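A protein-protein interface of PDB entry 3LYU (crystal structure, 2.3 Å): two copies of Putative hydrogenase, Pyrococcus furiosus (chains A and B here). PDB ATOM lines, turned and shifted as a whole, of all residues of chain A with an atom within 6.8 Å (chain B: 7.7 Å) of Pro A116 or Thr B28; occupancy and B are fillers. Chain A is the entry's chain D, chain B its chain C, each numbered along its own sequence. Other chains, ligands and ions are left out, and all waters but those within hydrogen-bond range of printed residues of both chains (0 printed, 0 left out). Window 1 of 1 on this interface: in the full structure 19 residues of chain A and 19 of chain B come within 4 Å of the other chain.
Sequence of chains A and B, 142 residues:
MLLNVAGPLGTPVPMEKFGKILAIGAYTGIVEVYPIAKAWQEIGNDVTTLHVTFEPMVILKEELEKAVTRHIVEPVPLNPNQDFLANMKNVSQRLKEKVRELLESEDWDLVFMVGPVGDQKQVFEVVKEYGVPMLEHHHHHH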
ATOM      1  N   ALA A  26     -35.974   0.471   5.862  1.00  0.00           N
ATOM      2  CA  ALA A  26     -35.438   1.805   5.669  1.00  0.00           C
ATOM      3  C   ALA A  26     -35.236   2.065   4.194  1.00  0.00           C
ATOM      4  O   ALA A  26     -34.706   1.220   3.477  1.00  0.00           O
ATOM      5  CB  ALA A  26     -34.119   1.953   6.408  1.00  0.00           C
ATOM      6  N   TYR A  27     -35.648   3.247   3.748  1.00  0.00           N
ATOM      7  CA  TYR A  27     -35.509   3.630   2.349  1.00  0.00           C
ATOM      8  C   TYR A  27     -36.191   2.578   1.467  1.00  0.00           C
ATOM      9  O   TYR A  27     -37.333   2.205   1.732  1.00  0.00           O
ATOM     10  CB  TYR A  27     -34.014   3.795   1.966  1.00  0.00           C
ATOM     11  CG  TYR A  27     -33.237   4.831   2.797  1.00  0.00           C
ATOM     12  CD1 TYR A  27     -32.391   4.432   3.837  1.00  0.00           C
ATOM     13  CD2 TYR A  27     -33.364   6.205   2.549  1.00  0.00           C
ATOM     14  CE1 TYR A  27     -31.700   5.362   4.593  1.00  0.00           C
ATOM     15  CE2 TYR A  27     -32.676   7.140   3.313  1.00  0.00           C
ATOM     16  CZ  TYR A  27     -31.848   6.707   4.329  1.00  0.00           C
ATOM     17  OH  TYR A  27     -31.156   7.614   5.087  1.00  0.00           O
ATOM     18  N   THR A  28     -35.510   2.096   0.432  1.00  0.00           N
ATOM     19  CA  THR A  28     -36.111   1.106  -0.466  1.00  0.00           C
ATOM     20  C   THR A  28     -36.118  -0.281   0.148  1.00  0.00           C
ATOM     21  O   THR A  28     -36.612  -1.229  -0.443  1.00  0.00           O
ATOM     22  CB  THR A  28     -35.368   1.030  -1.826  1.00  0.00           C
ATOM     23  OG1 THR A  28     -34.089   0.409  -1.650  1.00  0.00           O
ATOM     24  CG2 THR A  28     -35.156   2.441  -2.400  1.00  0.00           C
ATOM     25  N   GLY A  29     -35.558  -0.391   1.344  1.00  0.00           N
ATOM     26  CA  GLY A  29     -35.527  -1.666   2.022  1.00  0.00           C
ATOM     27  C   GLY A  29     -36.930  -2.174   2.272  1.00  0.00           C
ATOM     28  O   GLY A  29     -37.122  -3.361   2.476  1.00  0.00           O
ATOM     29  N   PHE A  54     -37.445   9.240   2.975  1.00  0.00           N
ATOM     30  CA  PHE A  54     -37.695  10.647   2.664  1.00  0.00           C
ATOM     31  C   PHE A  54     -39.070  10.818   2.066  1.00  0.00           C
ATOM     32  O   PHE A  54     -39.562   9.915   1.398  1.00  0.00           O
ATOM     33  CB  PHE A  54     -36.635  11.184   1.700  1.00  0.00           C
ATOM     34  CG  PHE A  54     -35.264  11.300   2.315  1.00  0.00           C
ATOM     35  CD1 PHE A  54     -35.061  12.081   3.453  1.00  0.00           C
ATOM     36  CD2 PHE A  54     -34.176  10.625   1.765  1.00  0.00           C
ATOM     37  CE1 PHE A  54     -33.799  12.187   4.037  1.00  0.00           C
ATOM     38  CE2 PHE A  54     -32.910  10.726   2.340  1.00  0.00           C
ATOM     39  CZ  PHE A  54     -32.721  11.508   3.480  1.00  0.00           C
ATOM     40  N   MET A  57     -40.180   9.360  -1.248  1.00  0.00           N
ATOM     41  CA  MET A  57     -39.801   7.969  -1.466  1.00  0.00           C
ATOM     42  C   MET A  57     -40.663   6.886  -0.838  1.00  0.00           C
ATOM     43  O   MET A  57     -40.293   5.706  -0.879  1.00  0.00           O
ATOM     44  CB  MET A  57     -38.369   7.753  -0.998  1.00  0.00           C
ATOM     45  CG  MET A  57     -37.335   8.499  -1.800  1.00  0.00           C
ATOM     46  SD  MET A  57     -35.593   8.124  -1.075  1.00  0.00           S
ATOM     47  CE  MET A  57     -35.651   6.179  -1.172  1.00  0.00           C
ATOM     48  N   PHE A  84     -26.140  14.764   0.808  1.00  0.00           N
ATOM     49  CA  PHE A  84     -27.040  13.684   1.167  1.00  0.00           C
ATOM     50  C   PHE A  84     -26.736  13.065   2.519  1.00  0.00           C
ATOM     51  O   PHE A  84     -27.625  12.544   3.179  1.00  0.00           O
ATOM     52  CB  PHE A  84     -27.018  12.612   0.091  1.00  0.00           C
ATOM     53  CG  PHE A  84     -28.191  11.709   0.144  1.00  0.00           C
ATOM     54  CD1 PHE A  84     -29.475  12.240   0.104  1.00  0.00           C
ATOM     55  CD2 PHE A  84     -28.024  10.333   0.267  1.00  0.00           C
ATOM     56  CE1 PHE A  84     -30.587  11.411   0.189  1.00  0.00           C
ATOM     57  CE2 PHE A  84     -29.124   9.487   0.353  1.00  0.00           C
ATOM     58  CZ  PHE A  84     -30.415  10.027   0.315  1.00  0.00           C
ATOM     59  N   MET A  88     -29.350  11.926   5.503  1.00  0.00           N
ATOM     60  CA  MET A  88     -29.529  10.568   5.974  1.00  0.00           C
ATOM     61  C   MET A  88     -29.489  10.572   7.484  1.00  0.00           C
ATOM     62  O   MET A  88     -30.133   9.754   8.141  1.00  0.00           O
ATOM     63  CB  MET A  88     -28.420   9.677   5.440  1.00  0.00           C
ATOM     64  CG  MET A  88     -28.395   9.570   3.932  1.00  0.00           C
ATOM     65  SD  MET A  88     -27.154   8.210   3.313  1.00  0.00           S
ATOM     66  CE  MET A  88     -28.052   6.648   3.938  1.00  0.00           C
ATOM     67  N   SER A  92     -31.801   8.577  10.059  1.00  0.00           N
ATOM     68  CA  SER A  92     -31.232   7.739  11.102  1.00  0.00           C
ATOM     69  C   SER A  92     -31.812   8.149  12.458  1.00  0.00           C
ATOM     70  O   SER A  92     -32.120   7.297  13.280  1.00  0.00           O
ATOM     71  CB  SER A  92     -29.708   7.878  11.127  1.00  0.00           C
ATOM     72  OG  SER A  92     -29.120   7.386   9.934  1.00  0.00           O
ATOM     73  N   MET A 113     -35.213  -6.145  10.533  1.00  0.00           N
ATOM     74  CA  MET A 113     -34.966  -4.972   9.731  1.00  0.00           C
ATOM     75  C   MET A 113     -34.109  -5.182   8.494  1.00  0.00           C
ATOM     76  O   MET A 113     -33.231  -6.039   8.453  1.00  0.00           O
ATOM     77  CB  MET A 113     -34.327  -3.877  10.579  1.00  0.00           C
ATOM     78  CG  MET A 113     -34.267  -2.541   9.847  1.00  0.00           C
ATOM     79  SD  MET A 113     -33.145  -1.181  10.652  1.00  0.00           S
ATOM     80  CE  MET A 113     -32.306  -0.560   9.040  1.00  0.00           C
ATOM     81  N   VAL A 114     -34.391  -4.374   7.480  1.00  0.00           N
ATOM     82  CA  VAL A 114     -33.648  -4.389   6.226  1.00  0.00           C
ATOM     83  C   VAL A 114     -33.420  -2.932   5.816  1.00  0.00           C
ATOM     84  O   VAL A 114     -34.370  -2.203   5.551  1.00  0.00           O
ATOM     85  CB  VAL A 114     -34.403  -5.173   5.095  1.00  0.00           C
ATOM     86  CG1 VAL A 114     -35.870  -4.854   5.123  1.00  0.00           C
ATOM     87  CG2 VAL A 114     -33.823  -4.813   3.734  1.00  0.00           C
ATOM     88  N   GLY A 115     -32.152  -2.528   5.800  1.00  0.00           N
ATOM     89  CA  GLY A 115     -31.775  -1.175   5.435  1.00  0.00           C
ATOM     90  C   GLY A 115     -30.260  -1.050   5.473  1.00  0.00           C
ATOM     91  O   GLY A 115     -29.577  -2.052   5.702  1.00  0.00           O
ATOM     92  N   PRO A 116     -29.691   0.150   5.237  1.00  0.00           N
ATOM     93  CA  PRO A 116     -28.232   0.255   5.280  1.00  0.00           C
ATOM     94  C   PRO A 116     -27.676  -0.298   6.590  1.00  0.00           C
ATOM     95  O   PRO A 116     -28.317  -0.199   7.644  1.00  0.00           O
ATOM     96  CB  PRO A 116     -27.975   1.759   5.082  1.00  0.00           C
ATOM     97  CG  PRO A 116     -29.274   2.412   5.386  1.00  0.00           C
ATOM     98  CD  PRO A 116     -30.294   1.439   4.864  1.00  0.00           C
ATOM     99  N   VAL A 117     -26.489  -0.896   6.517  1.00  0.00           N
ATOM    100  CA  VAL A 117     -25.850  -1.506   7.682  1.00  0.00           C
ATOM    101  C   VAL A 117     -25.512  -0.504   8.793  1.00  0.00           C
ATOM    102  O   VAL A 117     -25.213  -0.890   9.925  1.00  0.00           O
ATOM    103  CB  VAL A 117     -24.588  -2.287   7.243  1.00  0.00           C
ATOM    104  CG1 VAL A 117     -23.571  -1.344   6.664  1.00  0.00           C
ATOM    105  CG2 VAL A 117     -24.027  -3.066   8.406  1.00  0.00           C
ATOM    106  N   GLY A 118     -25.575   0.780   8.459  1.00  0.00           N
ATOM    107  CA  GLY A 118     -25.293   1.823   9.430  1.00  0.00           C
ATOM    108  C   GLY A 118     -26.509   2.106  10.298  1.00  0.00           C
ATOM    109  O   GLY A 118     -26.387   2.565  11.436  1.00  0.00           O
ATOM    110  N   ASP A 119     -27.690   1.833   9.749  1.00  0.00           N
ATOM    111  CA  ASP A 119     -28.932   2.042  10.471  1.00  0.00           C
ATOM    112  C   ASP A 119     -29.275   0.768  11.220  1.00  0.00           C
ATOM    113  O   ASP A 119     -29.912   0.800  12.270  1.00  0.00           O
ATOM    114  CB  ASP A 119     -30.060   2.407   9.504  1.00  0.00           C
ATOM    115  CG  ASP A 119     -29.872   3.778   8.887  1.00  0.00           C
ATOM    116  OD1 ASP A 119     -29.721   4.760   9.652  1.00  0.00           O
ATOM    117  OD2 ASP A 119     -29.877   3.879   7.645  1.00  0.00           O
ATOM    118  N   GLN A 120     -28.849  -0.360  10.671  1.00  0.00           N
ATOM    119  CA  GLN A 120     -29.108  -1.629  11.317  1.00  0.00           C
ATOM    120  C   GLN A 120     -28.363  -1.667  12.641  1.00  0.00           C
ATOM    121  O   GLN A 120     -28.829  -2.258  13.609  1.00  0.00           O
ATOM    122  CB  GLN A 120     -28.654  -2.775  10.421  1.00  0.00           C
ATOM    123  CG  GLN A 120     -29.414  -2.853   9.118  1.00  0.00           C
ATOM    124  CD  GLN A 120     -29.237  -4.182   8.437  1.00  0.00           C
ATOM    125  OE1 GLN A 120     -28.147  -4.527   7.998  1.00  0.00           O
ATOM    126  NE2 GLN A 120     -30.313  -4.946   8.354  1.00  0.00           N
ATOM    127  N   LYS A 121     -27.201  -1.027  12.674  1.00  0.00           N
ATOM    128  CA  LYS A 121     -26.396  -0.968  13.882  1.00  0.00           C
ATOM    129  C   LYS A 121     -27.076  -0.079  14.913  1.00  0.00           C
ATOM    130  O   LYS A 121     -27.252  -0.473  16.060  1.00  0.00           O
ATOM    131  CB  LYS A 121     -25.018  -0.392  13.580  1.00  0.00           C
ATOM    132  CG  LYS A 121     -24.125  -1.266  12.737  1.00  0.00           C
ATOM    133  CD  LYS A 121     -22.742  -0.649  12.647  1.00  0.00           C
ATOM    134  CE  LYS A 121     -21.755  -1.580  11.986  1.00  0.00           C
ATOM    135  NZ  LYS A 121     -20.386  -1.016  12.000  1.00  0.00           N
ATOM    136  N   HIS A 137     -30.436  -8.052   7.796  1.00  0.00           N
ATOM    137  CA  HIS A 137     -30.609  -8.413   6.383  1.00  0.00           C
ATOM    138  C   HIS A 137     -29.586  -9.507   6.017  1.00  0.00           C
ATOM    139  O   HIS A 137     -28.865 -10.003   6.928  1.00  0.00           O
ATOM    140  CB  HIS A 137     -30.382  -7.192   5.468  1.00  0.00           C
ATOM    141  CG  HIS A 137     -28.938  -6.947   5.124  1.00  0.00           C
ATOM    142  ND1 HIS A 137     -27.941  -6.876   6.077  1.00  0.00           N
ATOM    143  CD2 HIS A 137     -28.327  -6.759   3.929  1.00  0.00           C
ATOM    144  CE1 HIS A 137     -26.781  -6.656   5.487  1.00  0.00           C
ATOM    145  NE2 HIS A 137     -26.986  -6.581   4.183  1.00  0.00           N
ATOM    146  N   PRO B   8     -24.727  -6.145  13.834  1.00  0.00           N
ATOM    147  CA  PRO B   8     -24.604  -6.177  12.373  1.00  0.00           C
ATOM    148  C   PRO B   8     -23.346  -5.466  11.894  1.00  0.00           C
ATOM    149  O   PRO B   8     -23.011  -4.395  12.377  1.00  0.00           O
ATOM    150  CB  PRO B   8     -25.872  -5.478  11.905  1.00  0.00           C
ATOM    151  CG  PRO B   8     -26.119  -4.509  12.988  1.00  0.00           C
ATOM    152  CD  PRO B   8     -25.886  -5.332  14.232  1.00  0.00           C
ATOM    153  N   GLY B  25     -22.951   0.173  -6.336  1.00  0.00           N
ATOM    154  CA  GLY B  25     -23.707   0.558  -5.162  1.00  0.00           C
ATOM    155  C   GLY B  25     -24.967   1.263  -5.603  1.00  0.00           C
ATOM    156  O   GLY B  25     -24.898   2.326  -6.205  1.00  0.00           O
ATOM    157  N   ALA B  26     -26.118   0.668  -5.323  1.00  0.00           N
ATOM    158  CA  ALA B  26     -27.380   1.265  -5.711  1.00  0.00           C
ATOM    159  C   ALA B  26     -27.953   2.041  -4.531  1.00  0.00           C
ATOM    160  O   ALA B  26     -27.949   1.550  -3.396  1.00  0.00           O
ATOM    161  CB  ALA B  26     -28.343   0.186  -6.157  1.00  0.00           C
ATOM    162  N   TYR B  27     -28.447   3.247  -4.804  1.00  0.00           N
ATOM    163  CA  TYR B  27     -29.022   4.098  -3.772  1.00  0.00           C
ATOM    164  C   TYR B  27     -28.001   4.299  -2.647  1.00  0.00           C
ATOM    165  O   TYR B  27     -26.844   4.632  -2.922  1.00  0.00           O
ATOM    166  CB  TYR B  27     -30.332   3.488  -3.238  1.00  0.00           C
ATOM    167  CG  TYR B  27     -31.412   3.267  -4.299  1.00  0.00           C
ATOM    168  CD1 TYR B  27     -31.640   1.998  -4.834  1.00  0.00           C
ATOM    169  CD2 TYR B  27     -32.208   4.329  -4.766  1.00  0.00           C
ATOM    170  CE1 TYR B  27     -32.627   1.782  -5.801  1.00  0.00           C
ATOM    171  CE2 TYR B  27     -33.199   4.124  -5.734  1.00  0.00           C
ATOM    172  CZ  TYR B  27     -33.402   2.844  -6.248  1.00  0.00           C
ATOM    173  OH  TYR B  27     -34.362   2.615  -7.216  1.00  0.00           O
ATOM    174  N   THR B  28     -28.416   4.099  -1.395  1.00  0.00           N
ATOM    175  CA  THR B  28     -27.512   4.282  -0.253  1.00  0.00           C
ATOM    176  C   THR B  28     -26.555   3.107  -0.106  1.00  0.00           C
ATOM    177  O   THR B  28     -25.692   3.088   0.781  1.00  0.00           O
ATOM    178  CB  THR B  28     -28.284   4.451   1.089  1.00  0.00           C
ATOM    179  OG1 THR B  28     -28.878   3.204   1.476  1.00  0.00           O
ATOM    180  CG2 THR B  28     -29.370   5.496   0.953  1.00  0.00           C
ATOM    181  N   GLY B  29     -26.713   2.119  -0.977  1.00  0.00           N
ATOM    182  CA  GLY B  29     -25.836   0.972  -0.932  1.00  0.00           C
ATOM    183  C   GLY B  29     -24.388   1.371  -1.172  1.00  0.00           C
ATOM    184  O   GLY B  29     -23.470   0.633  -0.812  1.00  0.00           O
ATOM    185  N   ILE B  30     -24.177   2.543  -1.767  1.00  0.00           N
ATOM    186  CA  ILE B  30     -22.816   3.019  -2.055  1.00  0.00           C
ATOM    187  C   ILE B  30     -21.988   3.297  -0.788  1.00  0.00           C
ATOM    188  O   ILE B  30     -20.760   3.177  -0.800  1.00  0.00           O
ATOM    189  CB  ILE B  30     -22.836   4.291  -2.953  1.00  0.00           C
ATOM    190  CG1 ILE B  30     -21.474   4.475  -3.616  1.00  0.00           C
ATOM    191  CG2 ILE B  30     -23.176   5.518  -2.127  1.00  0.00           C
ATOM    192  CD1 ILE B  30     -21.113   3.356  -4.543  1.00  0.00           C
ATOM    193  N   VAL B  31     -22.668   3.653   0.299  1.00  0.00           N
ATOM    194  CA  VAL B  31     -22.007   3.927   1.574  1.00  0.00           C
ATOM    195  C   VAL B  31     -21.213   2.709   2.048  1.00  0.00           C
ATOM    196  O   VAL B  31     -20.084   2.816   2.540  1.00  0.00           O
ATOM    197  CB  VAL B  31     -23.052   4.281   2.651  1.00  0.00           C
ATOM    198  CG1 VAL B  31     -22.365   4.649   3.971  1.00  0.00           C
ATOM    199  CG2 VAL B  31     -23.912   5.423   2.152  1.00  0.00           C
ATOM    200  N   GLU B  32     -21.817   1.542   1.893  1.00  0.00           N
ATOM    201  CA  GLU B  32     -21.199   0.298   2.304  1.00  0.00           C
ATOM    202  C   GLU B  32     -20.107  -0.165   1.340  1.00  0.00           C
ATOM    203  O   GLU B  32     -19.056  -0.639   1.776  1.00  0.00           O
ATOM    204  CB  GLU B  32     -22.280  -0.778   2.445  1.00  0.00           C
ATOM    205  CG  GLU B  32     -21.814  -2.090   3.060  1.00  0.00           C
ATOM    206  CD  GLU B  32     -22.984  -3.006   3.438  1.00  0.00           C
ATOM    207  OE1 GLU B  32     -22.725  -4.155   3.866  1.00  0.00           O
ATOM    208  OE2 GLU B  32     -24.164  -2.576   3.314  1.00  0.00           O
ATOM    209  N   VAL B  33     -20.337  -0.038   0.035  1.00  0.00           N
ATOM    210  CA  VAL B  33     -19.320  -0.467  -0.914  1.00  0.00           C
ATOM    211  C   VAL B  33     -18.091   0.428  -0.831  1.00  0.00           C
ATOM    212  O   VAL B  33     -16.990  -0.012  -1.109  1.00  0.00           O
ATOM    213  CB  VAL B  33     -19.869  -0.534  -2.386  1.00  0.00           C
ATOM    214  CG1 VAL B  33     -21.094   0.316  -2.526  1.00  0.00           C
ATOM    215  CG2 VAL B  33     -18.802  -0.095  -3.386  1.00  0.00           C
ATOM    216  N   TYR B  34     -18.270   1.669  -0.409  1.00  0.00           N
ATOM    217  CA  TYR B  34     -17.132   2.573  -0.310  1.00  0.00           C
ATOM    218  C   TYR B  34     -15.922   1.976   0.410  1.00  0.00           C
ATOM    219  O   TYR B  34     -14.882   1.751  -0.219  1.00  0.00           O
ATOM    220  CB  TYR B  34     -17.537   3.885   0.361  1.00  0.00           C
ATOM    221  CG  TYR B  34     -16.376   4.811   0.636  1.00  0.00           C
ATOM    222  CD1 TYR B  34     -15.444   5.106  -0.355  1.00  0.00           C
ATOM    223  CD2 TYR B  34     -16.225   5.418   1.883  1.00  0.00           C
ATOM    224  CE1 TYR B  34     -14.387   5.983  -0.115  1.00  0.00           C
ATOM    225  CE2 TYR B  34     -15.172   6.302   2.136  1.00  0.00           C
ATOM    226  CZ  TYR B  34     -14.258   6.581   1.134  1.00  0.00           C
ATOM    227  OH  TYR B  34     -13.230   7.464   1.388  1.00  0.00           O
ATOM    228  N   HIS B  51     -22.201   4.176  -9.000  1.00  0.00           N
ATOM    229  CA  HIS B  51     -23.273   4.544  -8.090  1.00  0.00           C
ATOM    230  C   HIS B  51     -24.485   4.954  -8.901  1.00  0.00           C
ATOM    231  O   HIS B  51     -24.448   5.960  -9.597  1.00  0.00           O
ATOM    232  CB  HIS B  51     -22.869   5.718  -7.188  1.00  0.00           C
ATOM    233  CG  HIS B  51     -23.878   6.024  -6.118  1.00  0.00           C
ATOM    234  ND1 HIS B  51     -23.934   7.241  -5.471  1.00  0.00           N
ATOM    235  CD2 HIS B  51     -24.862   5.264  -5.573  1.00  0.00           C
ATOM    236  CE1 HIS B  51     -24.909   7.218  -4.577  1.00  0.00           C
ATOM    237  NE2 HIS B  51     -25.487   6.030  -4.617  1.00  0.00           N
ATOM    238  N   VAL B  52     -25.555   4.169  -8.830  1.00  0.00           N
ATOM    239  CA  VAL B  52     -26.770   4.503  -9.556  1.00  0.00           C
ATOM    240  C   VAL B  52     -27.813   4.864  -8.501  1.00  0.00           C
ATOM    241  O   VAL B  52     -28.152   4.046  -7.640  1.00  0.00           O
ATOM    242  CB  VAL B  52     -27.256   3.321 -10.402  1.00  0.00           C
ATOM    243  CG1 VAL B  52     -28.405   3.759 -11.271  1.00  0.00           C
ATOM    244  CG2 VAL B  52     -26.134   2.806 -11.259  1.00  0.00           C
ATOM    245  N   THR B  53     -28.296   6.102  -8.558  1.00  0.00           N
ATOM    246  CA  THR B  53     -29.288   6.599  -7.599  1.00  0.00           C
ATOM    247  C   THR B  53     -29.993   7.825  -8.182  1.00  0.00           C
ATOM    248  O   THR B  53     -29.778   8.176  -9.341  1.00  0.00           O
ATOM    249  CB  THR B  53     -28.607   6.971  -6.249  1.00  0.00           C
ATOM    250  OG1 THR B  53     -29.611   7.187  -5.253  1.00  0.00           O
ATOM    251  CG2 THR B  53     -27.736   8.211  -6.405  1.00  0.00           C
ATOM    252  N   MET B  57     -29.524  12.293  -4.412  1.00  0.00           N
ATOM    253  CA  MET B  57     -28.994  11.304  -3.476  1.00  0.00           C
ATOM    254  C   MET B  57     -27.554  10.834  -3.655  1.00  0.00           C
ATOM    255  O   MET B  57     -27.121   9.905  -2.970  1.00  0.00           O
ATOM    256  CB  MET B  57     -29.896  10.081  -3.479  1.00  0.00           C
ATOM    257  CG  MET B  57     -31.280  10.337  -2.953  1.00  0.00           C
ATOM    258  SD  MET B  57     -32.287   8.706  -3.017  1.00  0.00           S
ATOM    259  CE  MET B  57     -31.078   7.546  -2.018  1.00  0.00           C
ATOM    260  N   ILE B  59     -23.743  10.530  -3.059  1.00  0.00           N
ATOM    261  CA  ILE B  59     -22.931  10.769  -1.875  1.00  0.00           C
ATOM    262  C   ILE B  59     -21.574  10.096  -2.056  1.00  0.00           C
ATOM    263  O   ILE B  59     -21.434   9.184  -2.869  1.00  0.00           O
ATOM    264  CB  ILE B  59     -23.642  10.208  -0.597  1.00  0.00           C
ATOM    265  CG1 ILE B  59     -22.935  10.710   0.667  1.00  0.00           C
ATOM    266  CG2 ILE B  59     -23.690   8.678  -0.637  1.00  0.00           C
ATOM    267  CD1 ILE B  59     -22.969  12.227   0.832  1.00  0.00           C
ATOM    268  N   LEU B  60     -20.575  10.567  -1.311  1.00  0.00           N
ATOM    269  CA  LEU B  60     -19.223  10.011  -1.372  1.00  0.00           C
ATOM    270  C   LEU B  60     -18.518  10.112  -2.718  1.00  0.00           C
ATOM    271  O   LEU B  60     -17.443   9.536  -2.880  1.00  0.00           O
ATOM    272  CB  LEU B  60     -19.238   8.545  -0.951  1.00  0.00           C
ATOM    273  CG  LEU B  60     -18.961   8.205   0.511  1.00  0.00           C
ATOM    274  CD1 LEU B  60     -19.689   9.154   1.440  1.00  0.00           C
ATOM    275  CD2 LEU B  60     -19.396   6.773   0.752  1.00  0.00           C
ATOM    276  N   VAL B 114     -24.108  -4.104  -4.033  1.00  0.00           N
ATOM    277  CA  VAL B 114     -24.892  -3.937  -2.818  1.00  0.00           C
ATOM    278  C   VAL B 114     -26.029  -2.964  -3.136  1.00  0.00           C
ATOM    279  O   VAL B 114     -25.802  -1.809  -3.485  1.00  0.00           O
ATOM    280  CB  VAL B 114     -24.022  -3.416  -1.631  1.00  0.00           C
ATOM    281  CG1 VAL B 114     -23.077  -2.326  -2.098  1.00  0.00           C
ATOM    282  CG2 VAL B 114     -24.913  -2.892  -0.521  1.00  0.00           C
ATOM    283  N   GLY B 115     -27.255  -3.465  -3.041  1.00  0.00           N
ATOM    284  CA  GLY B 115     -28.436  -2.663  -3.315  1.00  0.00           C
ATOM    285  C   GLY B 115     -29.679  -3.520  -3.144  1.00  0.00           C
ATOM    286  O   GLY B 115     -29.554  -4.692  -2.763  1.00  0.00           O
ATOM    287  N   PRO B 116     -30.892  -2.984  -3.396  1.00  0.00           N
ATOM    288  CA  PRO B 116     -32.076  -3.838  -3.224  1.00  0.00           C
ATOM    289  C   PRO B 116     -31.941  -5.162  -3.964  1.00  0.00           C
ATOM    290  O   PRO B 116     -31.317  -5.226  -5.017  1.00  0.00           O
ATOM    291  CB  PRO B 116     -33.228  -2.966  -3.734  1.00  0.00           C
ATOM    292  CG  PRO B 116     -32.549  -1.889  -4.546  1.00  0.00           C
ATOM    293  CD  PRO B 116     -31.278  -1.623  -3.798  1.00  0.00           C
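The side-chain amide nitrogen (NE2) of Gln A120 lies within hydrogen-bond range of the backbone carbonyl oxygen (O) of Met A113.
The side-chain amide oxygen (OE1) of Gln A120 sits at hydrogen-bond distance from a ring nitrogen (ND1) of His A137 (3.0 Å).
The side-chain hydroxyl (OG) of Ser A92 is in hydrogen-bond range of the backbone carbonyl oxygen (O) of Met A88.
Among the printed residues, merely in contact across the chains: Met A57 with Met B57 (3.9 Å), Phe A84 with Met B57 (3.4 Å), Met A88 with Thr B28 (3.5 Å), Pro A116 with Thr B28 (3.99 Å), Val A117 with Glu B32 (3.6 Å), Gln A120 with Pro B8 (3.6 Å) and Lys A121 with Pro B8 (3.1 Å).
Printed residues of chain B within 4 Å of Phe A84: Met B57.
Of the printed residues of chain B, Pro A116 touches Thr B28 (3.99 Å).
Asp A119 touches none of the printed residues of chain B.
Printed residues of chain A within 4 Å of Thr B28: Met A88 and Pro A116.
Printed residues of chain A within 4 Å of Glu B32: Val A117.
Of the printed residues of chain A, Met B57 touches Met A57 and Phe A84.
The nearest printed residue of chain A that does not touch Thr B28 is Phe A84 (4.04 Å).
The nearest printed residue of chain A that does not touch Glu B32 is His A137 (4.9 Å).
Hydrophobic or aromatic side chains of chain B within 4 Å of the printed part of chain A: Pro B8 and Met B57.
Printed residues of chain A that touch a printed residue of chain B: Met A57, Phe A84, Met A88, Pro A116, Val A117, Gln A120 and Lys A121.
Along chain A the printed residues that touch a printed residue of chain B span positions 57 to 121.
Among the printed residues, 7 pairs touch across the chains.
Among the printed residues, no Asp or Glu carboxylate lies within 4 Å of a Lys or Arg side-chain nitrogen of the other chain.
Met A57 touches its own counterpart, Met B57.
Pro A116 touches Thr B28, but with the chains exchanged Thr A28 does not touch Pro B116 (4.005 Å).
Positions printed for both chains: 26, 27, 28, 29, 57, 114, 115 and 116.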
